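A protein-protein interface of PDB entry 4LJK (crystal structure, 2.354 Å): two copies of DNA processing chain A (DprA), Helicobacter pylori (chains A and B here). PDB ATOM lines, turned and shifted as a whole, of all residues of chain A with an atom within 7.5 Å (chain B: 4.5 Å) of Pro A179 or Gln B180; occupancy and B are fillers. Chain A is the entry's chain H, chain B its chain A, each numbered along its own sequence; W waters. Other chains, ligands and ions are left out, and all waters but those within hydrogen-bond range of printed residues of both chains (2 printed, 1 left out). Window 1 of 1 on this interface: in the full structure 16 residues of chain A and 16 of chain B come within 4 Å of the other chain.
Tyr A53 touches Arg B181, and with the chains exchanged Arg A181 touches Tyr B53. Pro A179 touches Gln B180, and with the chains exchanged Gln A180 touches Pro B179. Arg A181 touches its own counterpart, Arg B181. Leu A182 touches Pro B179, but with the chains exchanged Pro A179 does not touch Leu B182 (4.1 Å). Of the 14 pairs that touch across the chains among the printed residues, 7 have their exchanged pair printed and touching as well.
OH of Tyr B53 sits at hydrogen-bond distance from N of Leu A182. NH1 of Arg A181 lies close to NH1 of Arg B181 (3.4 Å). The guanidinium group (NH2) of Arg B181 lies within salt-bridge range of the side-chain carboxylate (OE1) of Glu A184, at 3.0 Å. The side-chain hydroxyl (OH) of Tyr A53 sits at hydrogen-bond distance from the backbone NH (N) of Leu B182 (3.0 Å).
Of the 22 printed residues of chain A, 10 touch a printed residue of chain B. Hydrophobic or aromatic side chains of chain A within 4 Å of the printed part of chain B: Tyr A53, His A57, Pro A179, Leu A182, Phe A201 and Ile A203. Of the 12 printed residues of chain B, 6 touch a printed residue of chain A. Printed residues of chain B that touch a printed residue of chain A: Tyr B53, Pro B179, Gln B180, Arg B181, Leu B182 and Asn B189. Hydrophobic or aromatic side chains of chain B within 4 Å of the printed part of chain A: Tyr B53, Pro B179 and Leu B182. Among the printed residues, 14 pairs touch across the chains.
Printed residues of chain B within 4 Å of Glu A184: Arg B181 (3.0 Å). Printed residues of chain B within 4 Å of Ile A200: Leu B182. Gln B154 touches none of the printed residues of chain A. Gln B180 touches one residue of chain A. The nearest residue of chain A that does not touch Gln B180 is Gln A180 (4.8 Å).
O of Gln B180 sits at hydrogen-bond distance from ND2 of Asn B189, 3.2 Å away. The side-chain amide nitrogen (NE2) of Gln A180 lies within hydrogen-bond range of the side-chain hydroxyl (OG) of Ser A54 (3.1 Å). O of Pro B153 sits at hydrogen-bond distance from NE2 of Gln B180, at 2.9 Å. OH of Tyr B53 is in hydrogen-bond range of O of Pro B179 (2.9 Å). N of Ile A200 lies close to O of Val A177 (3.1 Å). The side-chain amide nitrogen (ND2) of Asn A189 is in hydrogen-bond range of the backbone carbonyl oxygen (O) of Arg A181, at 3.4 Å.
Among the printed residues, merely in contact across the chains: Tyr A53 with Arg B181, His A57 with Leu B182, Pro A179 with Gln B180, Gln A180 with Pro B179, Arg A181 with Tyr B53, Leu A182 with Pro B179, Ile A200 with Leu B182, Phe A201 with Leu B182, Phe A201 with Asn B189 and Ile A203 with Leu B182.
Water W1 lies within hydrogen-bond range of NE of Arg A181 (2.5 Å), OE1 of Gln B180 (2.9 Å) and N of Arg B181 (3.4 Å). Water W2 bridges NE2 of His A57 and O of Leu B182.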
ATOM      1  N   TYR A  53       5.289  14.222 -18.286  1.00  0.00           N
ATOM      2  CA  TYR A  53       5.147  14.208 -16.843  1.00  0.00           C
ATOM      3  C   TYR A  53       6.308  14.939 -16.169  1.00  0.00           C
ATOM      4  O   TYR A  53       6.098  15.805 -15.333  1.00  0.00           O
ATOM      5  CB  TYR A  53       5.052  12.781 -16.323  1.00  0.00           C
ATOM      6  CG  TYR A  53       5.282  12.671 -14.836  1.00  0.00           C
ATOM      7  CD1 TYR A  53       4.331  13.127 -13.928  1.00  0.00           C
ATOM      8  CD2 TYR A  53       6.450  12.109 -14.340  1.00  0.00           C
ATOM      9  CE1 TYR A  53       4.545  13.025 -12.561  1.00  0.00           C
ATOM     10  CE2 TYR A  53       6.666  11.995 -12.984  1.00  0.00           C
ATOM     11  CZ  TYR A  53       5.712  12.452 -12.101  1.00  0.00           C
ATOM     12  OH  TYR A  53       5.940  12.342 -10.758  1.00  0.00           O
ATOM     13  N   SER A  54       7.525  14.588 -16.552  1.00  0.00           N
ATOM     14  CA  SER A  54       8.709  15.233 -16.010  1.00  0.00           C
ATOM     15  C   SER A  54       8.728  16.722 -16.339  1.00  0.00           C
ATOM     16  O   SER A  54       8.857  17.554 -15.450  1.00  0.00           O
ATOM     17  CB  SER A  54       9.960  14.530 -16.519  1.00  0.00           C
ATOM     18  OG  SER A  54       9.900  13.153 -16.175  1.00  0.00           O
ATOM     19  N   HIS A  57       6.306  19.086 -14.272  1.00  0.00           N
ATOM     20  CA  HIS A  57       6.694  19.396 -12.897  1.00  0.00           C
ATOM     21  C   HIS A  57       7.986  20.208 -12.831  1.00  0.00           C
ATOM     22  O   HIS A  57       8.202  20.982 -11.896  1.00  0.00           O
ATOM     23  CB  HIS A  57       6.775  18.119 -12.065  1.00  0.00           C
ATOM     24  CG  HIS A  57       5.456  17.435 -11.904  1.00  0.00           C
ATOM     25  ND1 HIS A  57       4.450  17.948 -11.115  1.00  0.00           N
ATOM     26  CD2 HIS A  57       4.970  16.292 -12.446  1.00  0.00           C
ATOM     27  CE1 HIS A  57       3.405  17.138 -11.163  1.00  0.00           C
ATOM     28  NE2 HIS A  57       3.692  16.130 -11.966  1.00  0.00           N
ATOM     29  N   ILE A 152      16.948  16.624  -9.936  1.00  0.00           N
ATOM     30  CA  ILE A 152      17.039  15.873 -11.177  1.00  0.00           C
ATOM     31  C   ILE A 152      15.676  15.238 -11.451  1.00  0.00           C
ATOM     32  O   ILE A 152      15.393  14.139 -10.966  1.00  0.00           O
ATOM     33  CB  ILE A 152      18.089  14.753 -11.090  1.00  0.00           C
ATOM     34  CG1 ILE A 152      19.441  15.305 -10.636  1.00  0.00           C
ATOM     35  CG2 ILE A 152      18.233  14.043 -12.420  1.00  0.00           C
ATOM     36  CD1 ILE A 152      20.533  14.259 -10.591  1.00  0.00           C
ATOM     37  N   PRO A 153      14.822  15.931 -12.224  1.00  0.00           N
ATOM     38  CA  PRO A 153      13.447  15.445 -12.427  1.00  0.00           C
ATOM     39  C   PRO A 153      13.384  14.031 -13.030  1.00  0.00           C
ATOM     40  O   PRO A 153      12.500  13.246 -12.671  1.00  0.00           O
ATOM     41  CB  PRO A 153      12.840  16.472 -13.400  1.00  0.00           C
ATOM     42  CG  PRO A 153      13.712  17.725 -13.233  1.00  0.00           C
ATOM     43  CD  PRO A 153      15.089  17.216 -12.909  1.00  0.00           C
ATOM     44  N   VAL A 177      14.960  14.138  -6.469  1.00  0.00           N
ATOM     45  CA  VAL A 177      14.425  13.614  -7.719  1.00  0.00           C
ATOM     46  C   VAL A 177      12.918  13.475  -7.666  1.00  0.00           C
ATOM     47  O   VAL A 177      12.333  13.343  -6.596  1.00  0.00           O
ATOM     48  CB  VAL A 177      14.997  12.233  -8.093  1.00  0.00           C
ATOM     49  CG1 VAL A 177      16.522  12.276  -8.138  1.00  0.00           C
ATOM     50  CG2 VAL A 177      14.463  11.149  -7.154  1.00  0.00           C
ATOM     51  N   LEU A 178      12.303  13.508  -8.842  1.00  0.00           N
ATOM     52  CA  LEU A 178      10.857  13.394  -8.967  1.00  0.00           C
ATOM     53  C   LEU A 178      10.477  11.921  -8.848  1.00  0.00           C
ATOM     54  O   LEU A 178      11.183  11.053  -9.355  1.00  0.00           O
ATOM     55  CB  LEU A 178      10.422  13.937 -10.336  1.00  0.00           C
ATOM     56  CG  LEU A 178       9.324  15.001 -10.447  1.00  0.00           C
ATOM     57  CD1 LEU A 178       9.501  16.145  -9.458  1.00  0.00           C
ATOM     58  CD2 LEU A 178       9.276  15.540 -11.868  1.00  0.00           C
ATOM     59  N   PRO A 179       9.356  11.625  -8.183  1.00  0.00           N
ATOM     60  CA  PRO A 179       8.967  10.208  -8.212  1.00  0.00           C
ATOM     61  C   PRO A 179       8.673   9.786  -9.658  1.00  0.00           C
ATOM     62  O   PRO A 179       8.016  10.535 -10.380  1.00  0.00           O
ATOM     63  CB  PRO A 179       7.689  10.169  -7.363  1.00  0.00           C
ATOM     64  CG  PRO A 179       7.618  11.491  -6.652  1.00  0.00           C
ATOM     65  CD  PRO A 179       8.365  12.475  -7.504  1.00  0.00           C
ATOM     66  N   GLN A 180       9.172   8.621 -10.068  1.00  0.00           N
ATOM     67  CA  GLN A 180       8.963   8.108 -11.415  1.00  0.00           C
ATOM     68  C   GLN A 180       8.599   6.632 -11.344  1.00  0.00           C
ATOM     69  O   GLN A 180       9.089   5.916 -10.473  1.00  0.00           O
ATOM     70  CB  GLN A 180      10.238   8.254 -12.254  1.00  0.00           C
ATOM     71  CG  GLN A 180      10.783   9.665 -12.361  1.00  0.00           C
ATOM     72  CD  GLN A 180      10.119  10.479 -13.449  1.00  0.00           C
ATOM     73  OE1 GLN A 180       9.356   9.954 -14.253  1.00  0.00           O
ATOM     74  NE2 GLN A 180      10.416  11.775 -13.482  1.00  0.00           N
ATOM     75  N   ARG A 181       7.752   6.179 -12.263  1.00  0.00           N
ATOM     76  CA  ARG A 181       7.420   4.761 -12.366  1.00  0.00           C
ATOM     77  C   ARG A 181       8.680   3.956 -12.639  1.00  0.00           C
ATOM     78  O   ARG A 181       9.633   4.468 -13.228  1.00  0.00           O
ATOM     79  CB  ARG A 181       6.411   4.511 -13.497  1.00  0.00           C
ATOM     80  CG  ARG A 181       4.974   4.865 -13.149  1.00  0.00           C
ATOM     81  CD  ARG A 181       4.046   4.673 -14.340  1.00  0.00           C
ATOM     82  NE  ARG A 181       2.698   5.151 -14.058  1.00  0.00           N
ATOM     83  CZ  ARG A 181       1.756   5.351 -14.981  1.00  0.00           C
ATOM     84  NH1 ARG A 181       2.008   5.123 -16.268  1.00  0.00           N
ATOM     85  NH2 ARG A 181       0.556   5.783 -14.613  1.00  0.00           N
ATOM     86  N   LEU A 182       8.684   2.697 -12.216  1.00  0.00           N
ATOM     87  CA  LEU A 182       9.796   1.802 -12.516  1.00  0.00           C
ATOM     88  C   LEU A 182      10.058   1.751 -14.021  1.00  0.00           C
ATOM     89  O   LEU A 182       9.116   1.753 -14.820  1.00  0.00           O
ATOM     90  CB  LEU A 182       9.498   0.401 -11.989  1.00  0.00           C
ATOM     91  CG  LEU A 182       9.384   0.307 -10.465  1.00  0.00           C
ATOM     92  CD1 LEU A 182       8.639  -0.953 -10.064  1.00  0.00           C
ATOM     93  CD2 LEU A 182      10.760   0.348  -9.819  1.00  0.00           C
ATOM     94  N   GLU A 184      11.077   3.896 -16.034  1.00  0.00           N
ATOM     95  CA  GLU A 184      10.874   5.136 -16.776  1.00  0.00           C
ATOM     96  C   GLU A 184      11.977   6.164 -16.512  1.00  0.00           C
ATOM     97  O   GLU A 184      12.234   7.054 -17.331  1.00  0.00           O
ATOM     98  CB  GLU A 184       9.509   5.738 -16.458  1.00  0.00           C
ATOM     99  CG  GLU A 184       8.343   4.984 -17.067  1.00  0.00           C
ATOM    100  CD  GLU A 184       7.100   5.851 -17.188  1.00  0.00           C
ATOM    101  OE1 GLU A 184       6.940   6.782 -16.369  1.00  0.00           O
ATOM    102  OE2 GLU A 184       6.288   5.616 -18.108  1.00  0.00           O
ATOM    103  N   SER A 185      12.628   6.037 -15.366  1.00  0.00           N
ATOM    104  CA  SER A 185      13.707   6.942 -15.023  1.00  0.00           C
ATOM    105  C   SER A 185      14.668   6.178 -14.134  1.00  0.00           C
ATOM    106  O   SER A 185      14.712   6.390 -12.916  1.00  0.00           O
ATOM    107  CB  SER A 185      13.138   8.160 -14.302  1.00  0.00           C
ATOM    108  OG  SER A 185      14.130   9.123 -14.030  1.00  0.00           O
ATOM    109  N   THR A 188      17.313   8.070 -11.732  1.00  0.00           N
ATOM    110  CA  THR A 188      16.786   8.676 -10.524  1.00  0.00           C
ATOM    111  C   THR A 188      16.266   7.604  -9.558  1.00  0.00           C
ATOM    112  O   THR A 188      16.367   7.750  -8.333  1.00  0.00           O
ATOM    113  CB  THR A 188      15.694   9.715 -10.842  1.00  0.00           C
ATOM    114  OG1 THR A 188      14.514   9.045 -11.285  1.00  0.00           O
ATOM    115  CG2 THR A 188      16.161  10.660 -11.943  1.00  0.00           C
ATOM    116  N   ASN A 189      15.727   6.513 -10.099  1.00  0.00           N
ATOM    117  CA  ASN A 189      15.306   5.409  -9.243  1.00  0.00           C
ATOM    118  C   ASN A 189      16.477   4.706  -8.544  1.00  0.00           C
ATOM    119  O   ASN A 189      16.339   4.273  -7.409  1.00  0.00           O
ATOM    120  CB  ASN A 189      14.411   4.411  -9.983  1.00  0.00           C
ATOM    121  CG  ASN A 189      12.941   4.828  -9.976  1.00  0.00           C
ATOM    122  OD1 ASN A 189      12.472   5.507  -9.055  1.00  0.00           O
ATOM    123  ND2 ASN A 189      12.210   4.428 -11.017  1.00  0.00           N
ATOM    124  N   LEU A 192      17.444   6.636  -5.674  1.00  0.00           N
ATOM    125  CA  LEU A 192      16.462   6.442  -4.615  1.00  0.00           C
ATOM    126  C   LEU A 192      16.664   5.128  -3.854  1.00  0.00           C
ATOM    127  O   LEU A 192      16.592   5.115  -2.623  1.00  0.00           O
ATOM    128  CB  LEU A 192      15.030   6.574  -5.143  1.00  0.00           C
ATOM    129  CG  LEU A 192      14.561   8.022  -5.285  1.00  0.00           C
ATOM    130  CD1 LEU A 192      13.130   8.073  -5.747  1.00  0.00           C
ATOM    131  CD2 LEU A 192      14.715   8.761  -3.969  1.00  0.00           C
ATOM    132  N   GLN A 198      16.783  12.177  -2.314  1.00  0.00           N
ATOM    133  CA  GLN A 198      15.523  12.364  -1.620  1.00  0.00           C
ATOM    134  C   GLN A 198      14.408  12.581  -2.654  1.00  0.00           C
ATOM    135  O   GLN A 198      14.614  13.264  -3.664  1.00  0.00           O
ATOM    136  CB  GLN A 198      15.650  13.590  -0.725  1.00  0.00           C
ATOM    137  CG  GLN A 198      14.518  13.814   0.250  1.00  0.00           C
ATOM    138  CD  GLN A 198      14.930  14.767   1.363  1.00  0.00           C
ATOM    139  OE1 GLN A 198      16.110  15.115   1.495  1.00  0.00           O
ATOM    140  NE2 GLN A 198      13.959  15.197   2.166  1.00  0.00           N
ATOM    141  N   GLY A 199      13.236  11.999  -2.413  1.00  0.00           N
ATOM    142  CA  GLY A 199      12.115  12.148  -3.327  1.00  0.00           C
ATOM    143  C   GLY A 199      11.298  13.391  -3.030  1.00  0.00           C
ATOM    144  O   GLY A 199      11.253  13.853  -1.891  1.00  0.00           O
ATOM    145  N   ILE A 200      10.662  13.942  -4.061  1.00  0.00           N
ATOM    146  CA  ILE A 200       9.773  15.087  -3.894  1.00  0.00           C
ATOM    147  C   ILE A 200       8.329  14.613  -3.999  1.00  0.00           C
ATOM    148  O   ILE A 200       7.736  14.600  -5.087  1.00  0.00           O
ATOM    149  CB  ILE A 200      10.030  16.157  -4.965  1.00  0.00           C
ATOM    150  CG1 ILE A 200      11.476  16.656  -4.880  1.00  0.00           C
ATOM    151  CG2 ILE A 200       9.030  17.313  -4.823  1.00  0.00           C
ATOM    152  CD1 ILE A 200      12.287  16.397  -6.129  1.00  0.00           C
ATOM    153  N   PHE A 201       7.763  14.224  -2.865  1.00  0.00           N
ATOM    154  CA  PHE A 201       6.457  13.578  -2.868  1.00  0.00           C
ATOM    155  C   PHE A 201       5.319  14.583  -2.766  1.00  0.00           C
ATOM    156  O   PHE A 201       4.148  14.219  -2.887  1.00  0.00           O
ATOM    157  CB  PHE A 201       6.396  12.495  -1.787  1.00  0.00           C
ATOM    158  CG  PHE A 201       7.526  11.500  -1.883  1.00  0.00           C
ATOM    159  CD1 PHE A 201       7.658  10.691  -3.002  1.00  0.00           C
ATOM    160  CD2 PHE A 201       8.474  11.401  -0.877  1.00  0.00           C
ATOM    161  CE1 PHE A 201       8.709   9.781  -3.110  1.00  0.00           C
ATOM    162  CE2 PHE A 201       9.525  10.489  -0.973  1.00  0.00           C
ATOM    163  CZ  PHE A 201       9.644   9.679  -2.088  1.00  0.00           C
ATOM    164  N   ASN A 202       5.675  15.853  -2.583  1.00  0.00           N
ATOM    165  CA  ASN A 202       4.706  16.936  -2.674  1.00  0.00           C
ATOM    166  C   ASN A 202       5.378  18.241  -3.065  1.00  0.00           C
ATOM    167  O   ASN A 202       6.144  18.797  -2.288  1.00  0.00           O
ATOM    168  CB  ASN A 202       3.952  17.113  -1.357  1.00  0.00           C
ATOM    169  CG  ASN A 202       2.771  18.054  -1.490  1.00  0.00           C
ATOM    170  OD1 ASN A 202       2.918  19.275  -1.409  1.00  0.00           O
ATOM    171  ND2 ASN A 202       1.589  17.489  -1.703  1.00  0.00           N
ATOM    172  N   ILE A 203       5.085  18.726  -4.269  1.00  0.00           N
ATOM    173  CA  ILE A 203       5.705  19.945  -4.781  1.00  0.00           C
ATOM    174  C   ILE A 203       5.596  21.115  -3.798  1.00  0.00           C
ATOM    175  O   ILE A 203       6.595  21.767  -3.491  1.00  0.00           O
ATOM    176  CB  ILE A 203       5.111  20.373  -6.146  1.00  0.00           C
ATOM    177  CG1 ILE A 203       5.362  19.306  -7.215  1.00  0.00           C
ATOM    178  CG2 ILE A 203       5.701  21.697  -6.584  1.00  0.00           C
ATOM    179  CD1 ILE A 203       6.811  19.143  -7.588  1.00  0.00           C
ATOM    180  N   TYR B  53      -0.035  -0.111 -15.063  1.00  0.00           N
ATOM    181  CA  TYR B  53       1.254  -0.027 -14.390  1.00  0.00           C
ATOM    182  C   TYR B  53       1.242  -0.796 -13.071  1.00  0.00           C
ATOM    183  O   TYR B  53       2.035  -1.704 -12.878  1.00  0.00           O
ATOM    184  CB  TYR B  53       1.634   1.420 -14.119  1.00  0.00           C
ATOM    185  CG  TYR B  53       2.856   1.556 -13.243  1.00  0.00           C
ATOM    186  CD1 TYR B  53       4.116   1.200 -13.720  1.00  0.00           C
ATOM    187  CD2 TYR B  53       2.756   2.048 -11.957  1.00  0.00           C
ATOM    188  CE1 TYR B  53       5.236   1.325 -12.938  1.00  0.00           C
ATOM    189  CE2 TYR B  53       3.877   2.178 -11.157  1.00  0.00           C
ATOM    190  CZ  TYR B  53       5.121   1.820 -11.652  1.00  0.00           C
ATOM    191  OH  TYR B  53       6.254   1.964 -10.859  1.00  0.00           O
ATOM    192  N   SER B  54       0.340  -0.429 -12.169  1.00  0.00           N
ATOM    193  CA  SER B  54       0.288  -1.078 -10.860  1.00  0.00           C
ATOM    194  C   SER B  54      -0.045  -2.573 -10.966  1.00  0.00           C
ATOM    195  O   SER B  54       0.508  -3.386 -10.226  1.00  0.00           O
ATOM    196  CB  SER B  54      -0.677  -0.350  -9.923  1.00  0.00           C
ATOM    197  OG  SER B  54      -0.319   1.012  -9.810  1.00  0.00           O
ATOM    198  N   PRO B 153       0.695  -1.675  -3.595  1.00  0.00           N
ATOM    199  CA  PRO B 153       1.175  -1.235  -4.906  1.00  0.00           C
ATOM    200  C   PRO B 153       0.671   0.165  -5.262  1.00  0.00           C
ATOM    201  O   PRO B 153       1.457   0.995  -5.738  1.00  0.00           O
ATOM    202  CB  PRO B 153       0.575  -2.277  -5.863  1.00  0.00           C
ATOM    203  CG  PRO B 153       0.372  -3.507  -5.006  1.00  0.00           C
ATOM    204  CD  PRO B 153      -0.040  -2.954  -3.667  1.00  0.00           C
ATOM    205  N   GLN B 154      -0.618   0.413  -5.030  1.00  0.00           N
ATOM    206  CA  GLN B 154      -1.251   1.688  -5.359  1.00  0.00           C
ATOM    207  C   GLN B 154      -2.473   1.873  -4.454  1.00  0.00           C
ATOM    208  O   GLN B 154      -3.099   0.889  -4.035  1.00  0.00           O
ATOM    209  CB  GLN B 154      -1.668   1.710  -6.843  1.00  0.00           C
ATOM    210  CG  GLN B 154      -2.395   2.992  -7.301  1.00  0.00           C
ATOM    211  CD  GLN B 154      -3.118   2.835  -8.639  1.00  0.00           C
ATOM    212  OE1 GLN B 154      -2.681   2.095  -9.524  1.00  0.00           O
ATOM    213  NE2 GLN B 154      -4.244   3.520  -8.778  1.00  0.00           N
ATOM    214  N   LEU B 178       4.873   0.719  -4.246  1.00  0.00           N
ATOM    215  CA  LEU B 178       5.395   0.884  -5.596  1.00  0.00           C
ATOM    216  C   LEU B 178       5.688   2.374  -5.853  1.00  0.00           C
ATOM    217  O   LEU B 178       4.955   3.252  -5.390  1.00  0.00           O
ATOM    218  CB  LEU B 178       4.357   0.364  -6.604  1.00  0.00           C
ATOM    219  CG  LEU B 178       4.720  -0.722  -7.617  1.00  0.00           C
ATOM    220  CD1 LEU B 178       5.535  -1.833  -7.003  1.00  0.00           C
ATOM    221  CD2 LEU B 178       3.453  -1.284  -8.217  1.00  0.00           C
ATOM    222  N   PRO B 179       6.773   2.666  -6.579  1.00  0.00           N
ATOM    223  CA  PRO B 179       6.962   4.040  -7.055  1.00  0.00           C
ATOM    224  C   PRO B 179       5.760   4.507  -7.881  1.00  0.00           C
ATOM    225  O   PRO B 179       5.286   3.781  -8.763  1.00  0.00           O
ATOM    226  CB  PRO B 179       8.196   3.927  -7.944  1.00  0.00           C
ATOM    227  CG  PRO B 179       8.903   2.700  -7.473  1.00  0.00           C
ATOM    228  CD  PRO B 179       7.846   1.761  -7.026  1.00  0.00           C
ATOM    229  N   GLN B 180       5.261   5.702  -7.591  1.00  0.00           N
ATOM    230  CA  GLN B 180       4.110   6.240  -8.316  1.00  0.00           C
ATOM    231  C   GLN B 180       4.280   7.739  -8.590  1.00  0.00           C
ATOM    232  O   GLN B 180       4.717   8.493  -7.719  1.00  0.00           O
ATOM    233  CB  GLN B 180       2.815   6.014  -7.519  1.00  0.00           C
ATOM    234  CG  GLN B 180       2.499   4.564  -7.204  1.00  0.00           C
ATOM    235  CD  GLN B 180       1.760   3.872  -8.340  1.00  0.00           C
ATOM    236  OE1 GLN B 180       1.466   4.481  -9.370  1.00  0.00           O
ATOM    237  NE2 GLN B 180       1.450   2.597  -8.152  1.00  0.00           N
ATOM    238  N   ARG B 181       3.911   8.173  -9.789  1.00  0.00           N
ATOM    239  CA  ARG B 181       3.953   9.589 -10.130  1.00  0.00           C
ATOM    240  C   ARG B 181       3.185  10.466  -9.147  1.00  0.00           C
ATOM    241  O   ARG B 181       2.296   9.994  -8.447  1.00  0.00           O
ATOM    242  CB  ARG B 181       3.367   9.788 -11.520  1.00  0.00           C
ATOM    243  CG  ARG B 181       4.238   9.264 -12.607  1.00  0.00           C
ATOM    244  CD  ARG B 181       3.444   9.124 -13.853  1.00  0.00           C
ATOM    245  NE  ARG B 181       4.305   8.981 -15.013  1.00  0.00           N
ATOM    246  CZ  ARG B 181       3.858   8.687 -16.225  1.00  0.00           C
ATOM    247  NH1 ARG B 181       2.559   8.496 -16.419  1.00  0.00           N
ATOM    248  NH2 ARG B 181       4.712   8.575 -17.232  1.00  0.00           N
ATOM    249  N   LEU B 182       3.527  11.751  -9.111  1.00  0.00           N
ATOM    250  CA  LEU B 182       2.744  12.741  -8.375  1.00  0.00           C
ATOM    251  C   LEU B 182       1.271  12.788  -8.800  1.00  0.00           C
ATOM    252  O   LEU B 182       0.961  12.782  -9.995  1.00  0.00           O
ATOM    253  CB  LEU B 182       3.358  14.125  -8.568  1.00  0.00           C
ATOM    254  CG  LEU B 182       4.697  14.323  -7.856  1.00  0.00           C
ATOM    255  CD1 LEU B 182       5.391  15.575  -8.357  1.00  0.00           C
ATOM    256  CD2 LEU B 182       4.481  14.392  -6.356  1.00  0.00           C
ATOM    257  N   SER B 185      -1.302   8.019  -7.043  1.00  0.00           N
ATOM    258  CA  SER B 185      -1.878   7.395  -5.858  1.00  0.00           C
ATOM    259  C   SER B 185      -1.382   8.149  -4.636  1.00  0.00           C
ATOM    260  O   SER B 185      -0.248   7.963  -4.190  1.00  0.00           O
ATOM    261  CB  SER B 185      -1.597   5.885  -5.784  1.00  0.00           C
ATOM    262  OG  SER B 185      -0.220   5.588  -5.640  1.00  0.00           O
ATOM    263  N   THR B 188      -0.280   6.151  -1.180  1.00  0.00           N
ATOM    264  CA  THR B 188       1.058   5.586  -1.072  1.00  0.00           C
ATOM    265  C   THR B 188       2.140   6.657  -1.138  1.00  0.00           C
ATOM    266  O   THR B 188       3.192   6.508  -0.520  1.00  0.00           O
ATOM    267  CB  THR B 188       1.332   4.514  -2.135  1.00  0.00           C
ATOM    268  OG1 THR B 188       1.325   5.121  -3.425  1.00  0.00           O
ATOM    269  CG2 THR B 188       0.279   3.404  -2.071  1.00  0.00           C
ATOM    270  N   ASN B 189       1.907   7.734  -1.883  1.00  0.00           N
ATOM    271  CA  ASN B 189       2.892   8.820  -1.872  1.00  0.00           C
ATOM    272  C   ASN B 189       2.907   9.543  -0.522  1.00  0.00           C
ATOM    273  O   ASN B 189       3.967   9.908  -0.046  1.00  0.00           O
ATOM    274  CB  ASN B 189       2.741   9.794  -3.052  1.00  0.00           C
ATOM    275  CG  ASN B 189       3.312   9.233  -4.363  1.00  0.00           C
ATOM    276  OD1 ASN B 189       4.348   8.556  -4.377  1.00  0.00           O
ATOM    277  ND2 ASN B 189       2.634   9.525  -5.470  1.00  0.00           N
HETATM  278  O   HOH W   1       2.091   6.029 -11.787  1.00  0.00           O
HETATM  279  O   HOH W   2       1.376  14.593 -12.180  1.00  0.00           O
